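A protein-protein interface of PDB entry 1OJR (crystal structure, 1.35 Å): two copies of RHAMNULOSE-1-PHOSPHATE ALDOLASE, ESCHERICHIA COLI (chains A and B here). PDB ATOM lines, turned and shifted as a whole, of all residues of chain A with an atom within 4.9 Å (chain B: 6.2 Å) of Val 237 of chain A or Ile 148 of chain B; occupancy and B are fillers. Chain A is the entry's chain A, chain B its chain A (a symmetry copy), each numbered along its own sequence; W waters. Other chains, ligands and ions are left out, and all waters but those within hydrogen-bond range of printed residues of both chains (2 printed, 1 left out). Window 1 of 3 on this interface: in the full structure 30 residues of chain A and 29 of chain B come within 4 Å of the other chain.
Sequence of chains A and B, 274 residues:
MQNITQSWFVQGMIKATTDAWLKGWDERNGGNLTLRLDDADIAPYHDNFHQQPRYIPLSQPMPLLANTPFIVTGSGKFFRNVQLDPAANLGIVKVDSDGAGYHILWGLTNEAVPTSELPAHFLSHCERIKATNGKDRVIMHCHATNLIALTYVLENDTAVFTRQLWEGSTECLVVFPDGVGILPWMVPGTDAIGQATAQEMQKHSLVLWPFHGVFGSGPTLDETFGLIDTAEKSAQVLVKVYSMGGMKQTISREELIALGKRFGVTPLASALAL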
ATOM      1  N   GLY A 168       0.237 -20.178  -7.206  1.00  0.00           N
ATOM      2  CA  GLY A 168       0.375 -20.915  -8.450  1.00  0.00           C
ATOM      3  C   GLY A 168      -0.611 -22.030  -8.725  1.00  0.00           C
ATOM      4  O   GLY A 168      -0.596 -22.589  -9.818  1.00  0.00           O
ATOM      5  N   SER A 169      -1.432 -22.383  -7.735  1.00  0.00           N
ATOM      6  CA  SER A 169      -2.541 -23.332  -7.918  1.00  0.00           C
ATOM      7  C   SER A 169      -3.406 -23.200  -6.679  1.00  0.00           C
ATOM      8  O   SER A 169      -2.901 -23.246  -5.563  1.00  0.00           O
ATOM      9  CB  SER A 169      -2.085 -24.786  -8.094  1.00  0.00           C
ATOM     10  OG  SER A 169      -1.572 -25.013  -9.397  1.00  0.00           O
ATOM     11  N   LYS A 233       3.599 -28.906  -9.493  1.00  0.00           N
ATOM     12  CA  LYS A 233       2.630 -28.430 -10.478  1.00  0.00           C
ATOM     13  C   LYS A 233       2.503 -26.905 -10.399  1.00  0.00           C
ATOM     14  O   LYS A 233       2.521 -26.190 -11.410  1.00  0.00           O
ATOM     15  CB  LYS A 233       1.263 -29.099 -10.264  1.00  0.00           C
ATOM     16  CG  LYS A 233       0.121 -28.502 -11.091  1.00  0.00           C
ATOM     17  CD  LYS A 233       0.310 -28.669 -12.600  1.00  0.00           C
ATOM     18  CE  LYS A 233      -0.989 -28.415 -13.359  1.00  0.00           C
ATOM     19  NZ  LYS A 233      -1.865 -29.627 -13.387  1.00  0.00           N
ATOM     20  N   SER A 234       2.359 -26.398  -9.187  1.00  0.00           N
ATOM     21  CA  SER A 234       2.327 -24.960  -8.997  1.00  0.00           C
ATOM     22  C   SER A 234       3.617 -24.333  -9.535  1.00  0.00           C
ATOM     23  O   SER A 234       3.582 -23.333 -10.243  1.00  0.00           O
ATOM     24  CB  SER A 234       2.153 -24.625  -7.520  1.00  0.00           C
ATOM     25  OG  SER A 234       2.117 -23.230  -7.352  1.00  0.00           O
ATOM     26  N   ALA A 235       4.760 -24.933  -9.219  1.00  0.00           N
ATOM     27  CA  ALA A 235       6.024 -24.414  -9.726  1.00  0.00           C
ATOM     28  C   ALA A 235       6.050 -24.409 -11.265  1.00  0.00           C
ATOM     29  O   ALA A 235       6.584 -23.481 -11.873  1.00  0.00           O
ATOM     30  CB  ALA A 235       7.191 -25.218  -9.175  1.00  0.00           C
ATOM     31  N   GLN A 236       5.511 -25.457 -11.882  1.00  0.00           N
ATOM     32  CA  GLN A 236       5.449 -25.543 -13.333  1.00  0.00           C
ATOM     33  C   GLN A 236       4.632 -24.390 -13.919  1.00  0.00           C
ATOM     34  O   GLN A 236       5.016 -23.760 -14.913  1.00  0.00           O
ATOM     35  CB  GLN A 236       4.843 -26.886 -13.741  1.00  0.00           C
ATOM     36  CG  GLN A 236       4.790 -27.077 -15.243  1.00  0.00           C
ATOM     37  CD  GLN A 236       4.163 -28.381 -15.668  1.00  0.00           C
ATOM     38  OE1 GLN A 236       3.571 -29.093 -14.849  1.00  0.00           O
ATOM     39  NE2 GLN A 236       4.277 -28.695 -16.958  1.00  0.00           N
ATOM     40  N   VAL A 237       3.495 -24.116 -13.294  1.00  0.00           N
ATOM     41  CA  VAL A 237       2.652 -23.002 -13.696  1.00  0.00           C
ATOM     42  C   VAL A 237       3.424 -21.688 -13.546  1.00  0.00           C
ATOM     43  O   VAL A 237       3.436 -20.851 -14.462  1.00  0.00           O
ATOM     44  CB  VAL A 237       1.346 -22.970 -12.871  1.00  0.00           C
ATOM     45  CG1 VAL A 237       0.603 -21.660 -13.059  1.00  0.00           C
ATOM     46  CG2 VAL A 237       0.465 -24.166 -13.238  1.00  0.00           C
ATOM     47  N   LEU A 238       4.089 -21.512 -12.408  1.00  0.00           N
ATOM     48  CA  LEU A 238       4.840 -20.287 -12.159  1.00  0.00           C
ATOM     49  C   LEU A 238       5.950 -20.082 -13.184  1.00  0.00           C
ATOM     50  O   LEU A 238       6.147 -18.978 -13.675  1.00  0.00           O
ATOM     51  CB  LEU A 238       5.422 -20.281 -10.746  1.00  0.00           C
ATOM     52  CG  LEU A 238       4.412 -20.191  -9.597  1.00  0.00           C
ATOM     53  CD1 LEU A 238       5.119 -20.368  -8.278  1.00  0.00           C
ATOM     54  CD2 LEU A 238       3.642 -18.864  -9.612  1.00  0.00           C
ATOM     55  N   VAL A 239       6.685 -21.139 -13.516  1.00  0.00           N
ATOM     56  CA  VAL A 239       7.757 -20.996 -14.488  1.00  0.00           C
ATOM     57  C   VAL A 239       7.176 -20.498 -15.820  1.00  0.00           C
ATOM     58  O   VAL A 239       7.758 -19.644 -16.475  1.00  0.00           O
ATOM     59  CB  VAL A 239       8.547 -22.304 -14.640  1.00  0.00           C
ATOM     60  CG1 VAL A 239       9.463 -22.252 -15.853  1.00  0.00           C
ATOM     61  CG2 VAL A 239       9.343 -22.588 -13.361  1.00  0.00           C
ATOM     62  N   LYS A 240       6.026 -21.029 -16.226  1.00  0.00           N
ATOM     63  CA  LYS A 240       5.378 -20.549 -17.444  1.00  0.00           C
ATOM     64  C   LYS A 240       4.999 -19.076 -17.328  1.00  0.00           C
ATOM     65  O   LYS A 240       5.275 -18.276 -18.234  1.00  0.00           O
ATOM     66  CB  LYS A 240       4.128 -21.365 -17.755  1.00  0.00           C
ATOM     67  CG  LYS A 240       4.388 -22.777 -18.234  1.00  0.00           C
ATOM     68  CD  LYS A 240       3.097 -23.583 -18.378  1.00  0.00           C
ATOM     69  CE  LYS A 240       3.358 -25.026 -18.786  1.00  0.00           C
ATOM     70  NZ  LYS A 240       3.835 -25.175 -20.203  1.00  0.00           N
ATOM     71  N   VAL A 241       4.355 -18.716 -16.222  1.00  0.00           N
ATOM     72  CA  VAL A 241       3.921 -17.336 -16.010  1.00  0.00           C
ATOM     73  C   VAL A 241       5.103 -16.367 -15.996  1.00  0.00           C
ATOM     74  O   VAL A 241       5.055 -15.311 -16.638  1.00  0.00           O
ATOM     75  CB  VAL A 241       3.088 -17.221 -14.718  1.00  0.00           C
ATOM     76  CG1 VAL A 241       2.787 -15.769 -14.374  1.00  0.00           C
ATOM     77  CG2 VAL A 241       1.788 -18.006 -14.846  1.00  0.00           C
ATOM     78  N   GLU B  27      -2.744 -33.766 -10.713  1.00  0.00           N
ATOM     79  CA  GLU B  27      -1.924 -34.021  -9.553  1.00  0.00           C
ATOM     80  C   GLU B  27      -2.815 -34.317  -8.357  1.00  0.00           C
ATOM     81  O   GLU B  27      -3.917 -33.768  -8.242  1.00  0.00           O
ATOM     82  CB  GLU B  27      -1.062 -32.788  -9.244  1.00  0.00           C
ATOM     83  CG  GLU B  27      -1.819 -31.536  -8.789  1.00  0.00           C
ATOM     84  CD  GLU B  27      -2.485 -30.718  -9.897  1.00  0.00           C
ATOM     85  OE1 GLU B  27      -3.071 -29.681  -9.542  1.00  0.00           O
ATOM     86  OE2 GLU B  27      -2.419 -31.075 -11.089  1.00  0.00           O
ATOM     87  N   CYS B 142     -10.499 -30.562 -14.793  1.00  0.00           N
ATOM     88  CA  CYS B 142      -9.100 -30.918 -14.591  1.00  0.00           C
ATOM     89  C   CYS B 142      -8.272 -29.654 -14.439  1.00  0.00           C
ATOM     90  O   CYS B 142      -8.756 -28.534 -14.672  1.00  0.00           O
ATOM     91  CB  CYS B 142      -8.582 -31.809 -15.702  1.00  0.00           C
ATOM     92  SG  CYS B 142      -8.526 -30.975 -17.248  1.00  0.00           S
ATOM     93  N   HIS B 143      -7.029 -29.835 -14.036  1.00  0.00           N
ATOM     94  CA  HIS B 143      -6.119 -28.727 -13.819  1.00  0.00           C
ATOM     95  C   HIS B 143      -5.191 -28.603 -15.026  1.00  0.00           C
ATOM     96  O   HIS B 143      -3.992 -28.863 -14.949  1.00  0.00           O
ATOM     97  CB  HIS B 143      -5.378 -28.924 -12.499  1.00  0.00           C
ATOM     98  CG  HIS B 143      -6.278 -28.923 -11.302  1.00  0.00           C
ATOM     99  ND1 HIS B 143      -5.828 -29.207 -10.030  1.00  0.00           N
ATOM    100  CD2 HIS B 143      -7.610 -28.693 -11.191  1.00  0.00           C
ATOM    101  CE1 HIS B 143      -6.846 -29.124  -9.184  1.00  0.00           C
ATOM    102  NE2 HIS B 143      -7.938 -28.817  -9.864  1.00  0.00           N
ATOM    103  N   ALA B 144      -5.778 -28.207 -16.148  1.00  0.00           N
ATOM    104  CA  ALA B 144      -5.061 -28.109 -17.413  1.00  0.00           C
ATOM    105  C   ALA B 144      -3.993 -27.020 -17.304  1.00  0.00           C
ATOM    106  O   ALA B 144      -4.300 -25.832 -17.193  1.00  0.00           O
ATOM    107  CB  ALA B 144      -6.043 -27.820 -18.531  1.00  0.00           C
ATOM    108  N   THR B 145      -2.740 -27.443 -17.369  1.00  0.00           N
ATOM    109  CA  THR B 145      -1.600 -26.610 -16.993  1.00  0.00           C
ATOM    110  C   THR B 145      -1.460 -25.279 -17.699  1.00  0.00           C
ATOM    111  O   THR B 145      -1.288 -24.240 -17.057  1.00  0.00           O
ATOM    112  CB  THR B 145      -0.339 -27.439 -17.230  1.00  0.00           C
ATOM    113  OG1 THR B 145      -0.530 -28.731 -16.649  1.00  0.00           O
ATOM    114  CG2 THR B 145       0.874 -26.833 -16.534  1.00  0.00           C
ATOM    115  N   ASN B 146      -1.508 -25.300 -19.027  1.00  0.00           N
ATOM    116  CA  ASN B 146      -1.334 -24.076 -19.793  1.00  0.00           C
ATOM    117  C   ASN B 146      -2.515 -23.128 -19.664  1.00  0.00           C
ATOM    118  O   ASN B 146      -2.335 -21.916 -19.571  1.00  0.00           O
ATOM    119  CB  ASN B 146      -1.010 -24.409 -21.239  1.00  0.00           C
ATOM    120  CG  ASN B 146       0.352 -25.044 -21.370  1.00  0.00           C
ATOM    121  OD1 ASN B 146       1.375 -24.359 -21.263  1.00  0.00           O
ATOM    122  ND2 ASN B 146       0.386 -26.360 -21.581  1.00  0.00           N
ATOM    123  N   LEU B 147      -3.725 -23.671 -19.643  1.00  0.00           N
ATOM    124  CA  LEU B 147      -4.896 -22.838 -19.407  1.00  0.00           C
ATOM    125  C   LEU B 147      -4.765 -22.128 -18.056  1.00  0.00           C
ATOM    126  O   LEU B 147      -5.083 -20.949 -17.941  1.00  0.00           O
ATOM    127  CB  LEU B 147      -6.178 -23.680 -19.456  1.00  0.00           C
ATOM    128  CG  LEU B 147      -6.634 -24.049 -20.876  1.00  0.00           C
ATOM    129  CD1 LEU B 147      -7.679 -25.125 -20.840  1.00  0.00           C
ATOM    130  CD2 LEU B 147      -7.153 -22.855 -21.628  1.00  0.00           C
ATOM    131  N   ILE B 148      -4.310 -22.847 -17.036  1.00  0.00           N
ATOM    132  CA  ILE B 148      -4.118 -22.240 -15.729  1.00  0.00           C
ATOM    133  C   ILE B 148      -3.111 -21.115 -15.810  1.00  0.00           C
ATOM    134  O   ILE B 148      -3.370 -20.022 -15.363  1.00  0.00           O
ATOM    135  CB  ILE B 148      -3.663 -23.295 -14.695  1.00  0.00           C
ATOM    136  CG1 ILE B 148      -4.776 -24.297 -14.385  1.00  0.00           C
ATOM    137  CG2 ILE B 148      -3.224 -22.620 -13.393  1.00  0.00           C
ATOM    138  CD1 ILE B 148      -4.259 -25.554 -13.696  1.00  0.00           C
ATOM    139  N   ALA B 149      -1.967 -21.361 -16.437  1.00  0.00           N
ATOM    140  CA  ALA B 149      -0.948 -20.344 -16.569  1.00  0.00           C
ATOM    141  C   ALA B 149      -1.488 -19.097 -17.265  1.00  0.00           C
ATOM    142  O   ALA B 149      -1.198 -17.963 -16.866  1.00  0.00           O
ATOM    143  CB  ALA B 149       0.253 -20.900 -17.333  1.00  0.00           C
ATOM    144  N   LEU B 150      -2.284 -19.299 -18.308  1.00  0.00           N
ATOM    145  CA  LEU B 150      -2.822 -18.160 -19.036  1.00  0.00           C
ATOM    146  C   LEU B 150      -3.737 -17.293 -18.169  1.00  0.00           C
ATOM    147  O   LEU B 150      -3.867 -16.104 -18.426  1.00  0.00           O
ATOM    148  CB  LEU B 150      -3.562 -18.600 -20.301  1.00  0.00           C
ATOM    149  CG  LEU B 150      -2.669 -19.117 -21.416  1.00  0.00           C
ATOM    150  CD1 LEU B 150      -3.542 -19.497 -22.581  1.00  0.00           C
ATOM    151  CD2 LEU B 150      -1.618 -18.107 -21.844  1.00  0.00           C
ATOM    152  N   THR B 151      -4.392 -17.865 -17.161  1.00  0.00           N
ATOM    153  CA  THR B 151      -5.261 -17.039 -16.318  1.00  0.00           C
ATOM    154  C   THR B 151      -4.508 -16.011 -15.484  1.00  0.00           C
ATOM    155  O   THR B 151      -5.132 -15.114 -14.925  1.00  0.00           O
ATOM    156  CB  THR B 151      -6.207 -17.861 -15.411  1.00  0.00           C
ATOM    157  OG1 THR B 151      -5.463 -18.645 -14.458  1.00  0.00           O
ATOM    158  CG2 THR B 151      -7.069 -18.823 -16.224  1.00  0.00           C
ATOM    159  N   TYR B 152      -3.183 -16.135 -15.389  1.00  0.00           N
ATOM    160  CA  TYR B 152      -2.379 -15.139 -14.681  1.00  0.00           C
ATOM    161  C   TYR B 152      -1.904 -14.020 -15.602  1.00  0.00           C
ATOM    162  O   TYR B 152      -1.392 -13.017 -15.115  1.00  0.00           O
ATOM    163  CB  TYR B 152      -1.132 -15.773 -14.033  1.00  0.00           C
ATOM    164  CG  TYR B 152      -1.441 -16.811 -12.977  1.00  0.00           C
ATOM    165  CD1 TYR B 152      -1.706 -18.115 -13.342  1.00  0.00           C
ATOM    166  CD2 TYR B 152      -1.435 -16.498 -11.625  1.00  0.00           C
ATOM    167  CE1 TYR B 152      -2.012 -19.065 -12.419  1.00  0.00           C
ATOM    168  CE2 TYR B 152      -1.738 -17.463 -10.675  1.00  0.00           C
ATOM    169  CZ  TYR B 152      -2.019 -18.753 -11.093  1.00  0.00           C
ATOM    170  OH  TYR B 152      -2.315 -19.740 -10.195  1.00  0.00           O
ATOM    171  N   VAL B 153      -2.018 -14.207 -16.920  1.00  0.00           N
ATOM    172  CA  VAL B 153      -1.458 -13.240 -17.869  1.00  0.00           C
ATOM    173  C   VAL B 153      -2.453 -12.625 -18.854  1.00  0.00           C
ATOM    174  O   VAL B 153      -2.268 -11.488 -19.269  1.00  0.00           O
ATOM    175  CB  VAL B 153      -0.234 -13.835 -18.636  1.00  0.00           C
ATOM    176  CG1 VAL B 153       0.825 -14.301 -17.664  1.00  0.00           C
ATOM    177  CG2 VAL B 153      -0.613 -14.963 -19.562  1.00  0.00           C
ATOM    178  N   LEU B 208     -13.694 -21.597 -17.304  1.00  0.00           N
ATOM    179  CA  LEU B 208     -12.438 -21.498 -16.591  1.00  0.00           C
ATOM    180  C   LEU B 208     -12.629 -20.976 -15.178  1.00  0.00           C
ATOM    181  O   LEU B 208     -13.426 -20.066 -14.923  1.00  0.00           O
ATOM    182  CB  LEU B 208     -11.477 -20.566 -17.323  1.00  0.00           C
ATOM    183  CG  LEU B 208     -10.866 -21.118 -18.607  1.00  0.00           C
ATOM    184  CD1 LEU B 208     -10.195 -20.019 -19.392  1.00  0.00           C
ATOM    185  CD2 LEU B 208      -9.881 -22.240 -18.305  1.00  0.00           C
ATOM    186  N   TRP B 209     -11.883 -21.594 -14.277  1.00  0.00           N
ATOM    187  CA  TRP B 209     -11.758 -21.193 -12.893  1.00  0.00           C
ATOM    188  C   TRP B 209     -10.347 -20.618 -12.782  1.00  0.00           C
ATOM    189  O   TRP B 209      -9.374 -21.369 -12.802  1.00  0.00           O
ATOM    190  CB  TRP B 209     -11.904 -22.424 -11.995  1.00  0.00           C
ATOM    191  CG  TRP B 209     -13.300 -22.923 -11.797  1.00  0.00           C
ATOM    192  CD1 TRP B 209     -14.430 -22.514 -12.447  1.00  0.00           C
ATOM    193  CD2 TRP B 209     -13.717 -23.915 -10.855  1.00  0.00           C
ATOM    194  NE1 TRP B 209     -15.523 -23.206 -11.975  1.00  0.00           N
ATOM    195  CE2 TRP B 209     -15.115 -24.058 -10.983  1.00  0.00           C
ATOM    196  CE3 TRP B 209     -13.052 -24.688  -9.900  1.00  0.00           C
ATOM    197  CZ2 TRP B 209     -15.851 -24.944 -10.198  1.00  0.00           C
ATOM    198  CZ3 TRP B 209     -13.779 -25.571  -9.127  1.00  0.00           C
ATOM    199  CH2 TRP B 209     -15.172 -25.681  -9.271  1.00  0.00           C
ATOM    200  N   PRO B 210     -10.210 -19.299 -12.691  1.00  0.00           N
ATOM    201  CA  PRO B 210      -8.873 -18.689 -12.674  1.00  0.00           C
ATOM    202  C   PRO B 210      -7.990 -19.246 -11.573  1.00  0.00           C
ATOM    203  O   PRO B 210      -8.459 -19.496 -10.474  1.00  0.00           O
ATOM    204  CB  PRO B 210      -9.159 -17.204 -12.436  1.00  0.00           C
ATOM    205  CG  PRO B 210     -10.531 -16.998 -12.885  1.00  0.00           C
ATOM    206  CD  PRO B 210     -11.271 -18.282 -12.634  1.00  0.00           C
ATOM    207  N   PHE B 211      -6.726 -19.471 -11.904  1.00  0.00           N
ATOM    208  CA  PHE B 211      -5.747 -19.922 -10.929  1.00  0.00           C
ATOM    209  C   PHE B 211      -6.104 -21.307 -10.399  1.00  0.00           C
ATOM    210  O   PHE B 211      -5.651 -21.704  -9.326  1.00  0.00           O
ATOM    211  CB  PHE B 211      -5.625 -18.919  -9.766  1.00  0.00           C
ATOM    212  CG  PHE B 211      -5.782 -17.468 -10.170  1.00  0.00           C
ATOM    213  CD1 PHE B 211      -6.635 -16.631  -9.460  1.00  0.00           C
ATOM    214  CD2 PHE B 211      -5.077 -16.927 -11.239  1.00  0.00           C
ATOM    215  CE1 PHE B 211      -6.786 -15.307  -9.804  1.00  0.00           C
ATOM    216  CE2 PHE B 211      -5.252 -15.596 -11.600  1.00  0.00           C
ATOM    217  CZ  PHE B 211      -6.096 -14.787 -10.867  1.00  0.00           C
ATOM    218  N   HIS B 212      -6.882 -22.055 -11.172  1.00  0.00           N
ATOM    219  CA  HIS B 212      -7.369 -23.347 -10.720  1.00  0.00           C
ATOM    220  C   HIS B 212      -7.501 -24.366 -11.850  1.00  0.00           C
ATOM    221  O   HIS B 212      -6.824 -25.380 -11.838  1.00  0.00           O
ATOM    222  CB  HIS B 212      -8.694 -23.168  -9.971  1.00  0.00           C
ATOM    223  CG  HIS B 212      -9.210 -24.423  -9.341  1.00  0.00           C
ATOM    224  ND1 HIS B 212     -10.029 -24.407  -8.234  1.00  0.00           N
ATOM    225  CD2 HIS B 212      -9.055 -25.730  -9.674  1.00  0.00           C
ATOM    226  CE1 HIS B 212     -10.351 -25.646  -7.908  1.00  0.00           C
ATOM    227  NE2 HIS B 212      -9.771 -26.469  -8.765  1.00  0.00           N
ATOM    228  N   GLY B 213      -8.386 -24.131 -12.811  1.00  0.00           N
ATOM    229  CA  GLY B 213      -8.567 -25.112 -13.848  1.00  0.00           C
ATOM    230  C   GLY B 213      -9.725 -24.857 -14.768  1.00  0.00           C
ATOM    231  O   GLY B 213     -10.146 -23.724 -14.953  1.00  0.00           O
ATOM    232  N   VAL B 214     -10.246 -25.939 -15.337  1.00  0.00           N
ATOM    233  CA  VAL B 214     -11.265 -25.848 -16.358  1.00  0.00           C
ATOM    234  C   VAL B 214     -12.342 -26.896 -16.156  1.00  0.00           C
ATOM    235  O   VAL B 214     -12.089 -27.963 -15.587  1.00  0.00           O
ATOM    236  CB  VAL B 214     -10.610 -26.009 -17.762  1.00  0.00           C
ATOM    237  CG1 VAL B 214     -10.055 -27.423 -17.971  1.00  0.00           C
ATOM    238  CG2 VAL B 214     -11.565 -25.620 -18.869  1.00  0.00           C
ATOM    239  N   GLU B 232      -6.599 -26.833 -24.280  1.00  0.00           N
ATOM    240  CA  GLU B 232      -5.311 -26.890 -23.613  1.00  0.00           C
ATOM    241  C   GLU B 232      -4.142 -26.916 -24.601  1.00  0.00           C
ATOM    242  O   GLU B 232      -3.074 -26.363 -24.316  1.00  0.00           O
ATOM    243  CB  GLU B 232      -5.277 -28.084 -22.663  1.00  0.00           C
ATOM    244  CG  GLU B 232      -3.929 -28.376 -22.021  1.00  0.00           C
ATOM    245  CD  GLU B 232      -3.382 -27.290 -21.112  1.00  0.00           C
ATOM    246  OE1 GLU B 232      -2.193 -27.431 -20.737  1.00  0.00           O
ATOM    247  OE2 GLU B 232      -4.096 -26.318 -20.772  1.00  0.00           O
HETATM  248  O   HOH W   1      -2.906 -27.094 -10.711  1.00  0.00           O
HETATM  249  O   HOH W   2       3.787 -24.223 -23.516  1.00  0.00           O
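Printed residues of chain A within 4 Å of Ile 148 of chain B: Val 237 (3.96 Å). Of the printed residues of chain A, Asn 146 of chain B touches Lys 240 (2.8 Å). Printed residues of chain A within 4 Å of His 143 of chain B: Lys 233. Glu 232 of chain B touches none of the printed residues of chain A. Leu 150 of chain B touches none of the printed residues of chain A. The nearest residue of chain B that does not touch Val 237 of chain A is Ala 149 of chain B (4.1 Å). The nearest printed residue of chain A that does not touch Ile 148 of chain B is Lys 233 of chain A (4.4 Å). The nearest printed residue of chain B that does not touch Gln 236 of chain A is Ala 149 of chain B (6.1 Å).
Ser 169 of chain A touches Tyr 152 of chain B (N to OH, 3.7 Å). Phe 211 of chain B touches Ser 169 of chain A (O to C, 3.8 Å). Thr 145 of chain B touches Lys 233 of chain A (OG1 to CE, 3.3 Å). Gln 236 of chain A touches Thr 145 of chain B (CD to CG2, 3.7 Å). Val 237 of chain A touches Ile 148 of chain B. Val 237 of chain A touches Tyr 152 of chain B. Thr 145 of chain B touches Lys 240 of chain A. Lys 240 of chain A touches Ala 149 of chain B (CB to CB, 3.9 Å). O of Ala 149 of chain B touches CG2 of Val 241 of chain A, at 3.6 Å. CB of Tyr 152 of chain B touches CG2 of Val 241 of chain A (3.8 Å).
OE1 of Glu 27 of chain B sits at hydrogen-bond distance from ND1 of His 143 of chain B (2.8 Å). O of Ile 148 of chain B lies within hydrogen-bond range of OG1 of Thr 151 of chain B. OE1 of Glu 232 of chain B sits at hydrogen-bond distance from N of Thr 145 of chain B. OE1 of Glu 232 of chain B lies within hydrogen-bond range of N of Asn 146 of chain B (2.8 Å). The backbone NH (N) of Phe 211 of chain B lies within hydrogen-bond range of the side-chain hydroxyl (OG1) of Thr 151 of chain B.
No position is printed for both chains.
Water W1 bridges OG of Ser 169 of chain A and OE1 of Glu 27 of chain B. Water W2 bridges OD1 of Asn 146 of chain B (3.3 Å) and NZ of Lys 240 of chain A (3.4 Å).
Of the 21 printed residues of chain B, 8 touch a printed residue of chain A. Printed residues of chain B that touch a printed residue of chain A: Glu 27, His 143, Thr 145, Asn 146, Ile 148, Ala 149, Tyr 152 and Phe 211. Of the 11 printed residues of chain A, 7 touch a printed residue of chain B. Among the printed residues, 14 pairs touch across the chains.
OE2 of Glu 27 of chain B lies within salt-bridge range of NZ of Lys 233 of chain A, at 2.8 Å. NZ of Lys 240 of chain A sits at hydrogen-bond distance from OD1 of Asn 146 of chain B, 2.8 Å away. NZ of Lys 233 of chain A sits at hydrogen-bond distance from O of His 143 of chain B (2.7 Å). The backbone carbonyl oxygen of Gly 168 of chain A lies close to the side-chain hydroxyl of Tyr 152 of chain B, 3.3 Å away.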
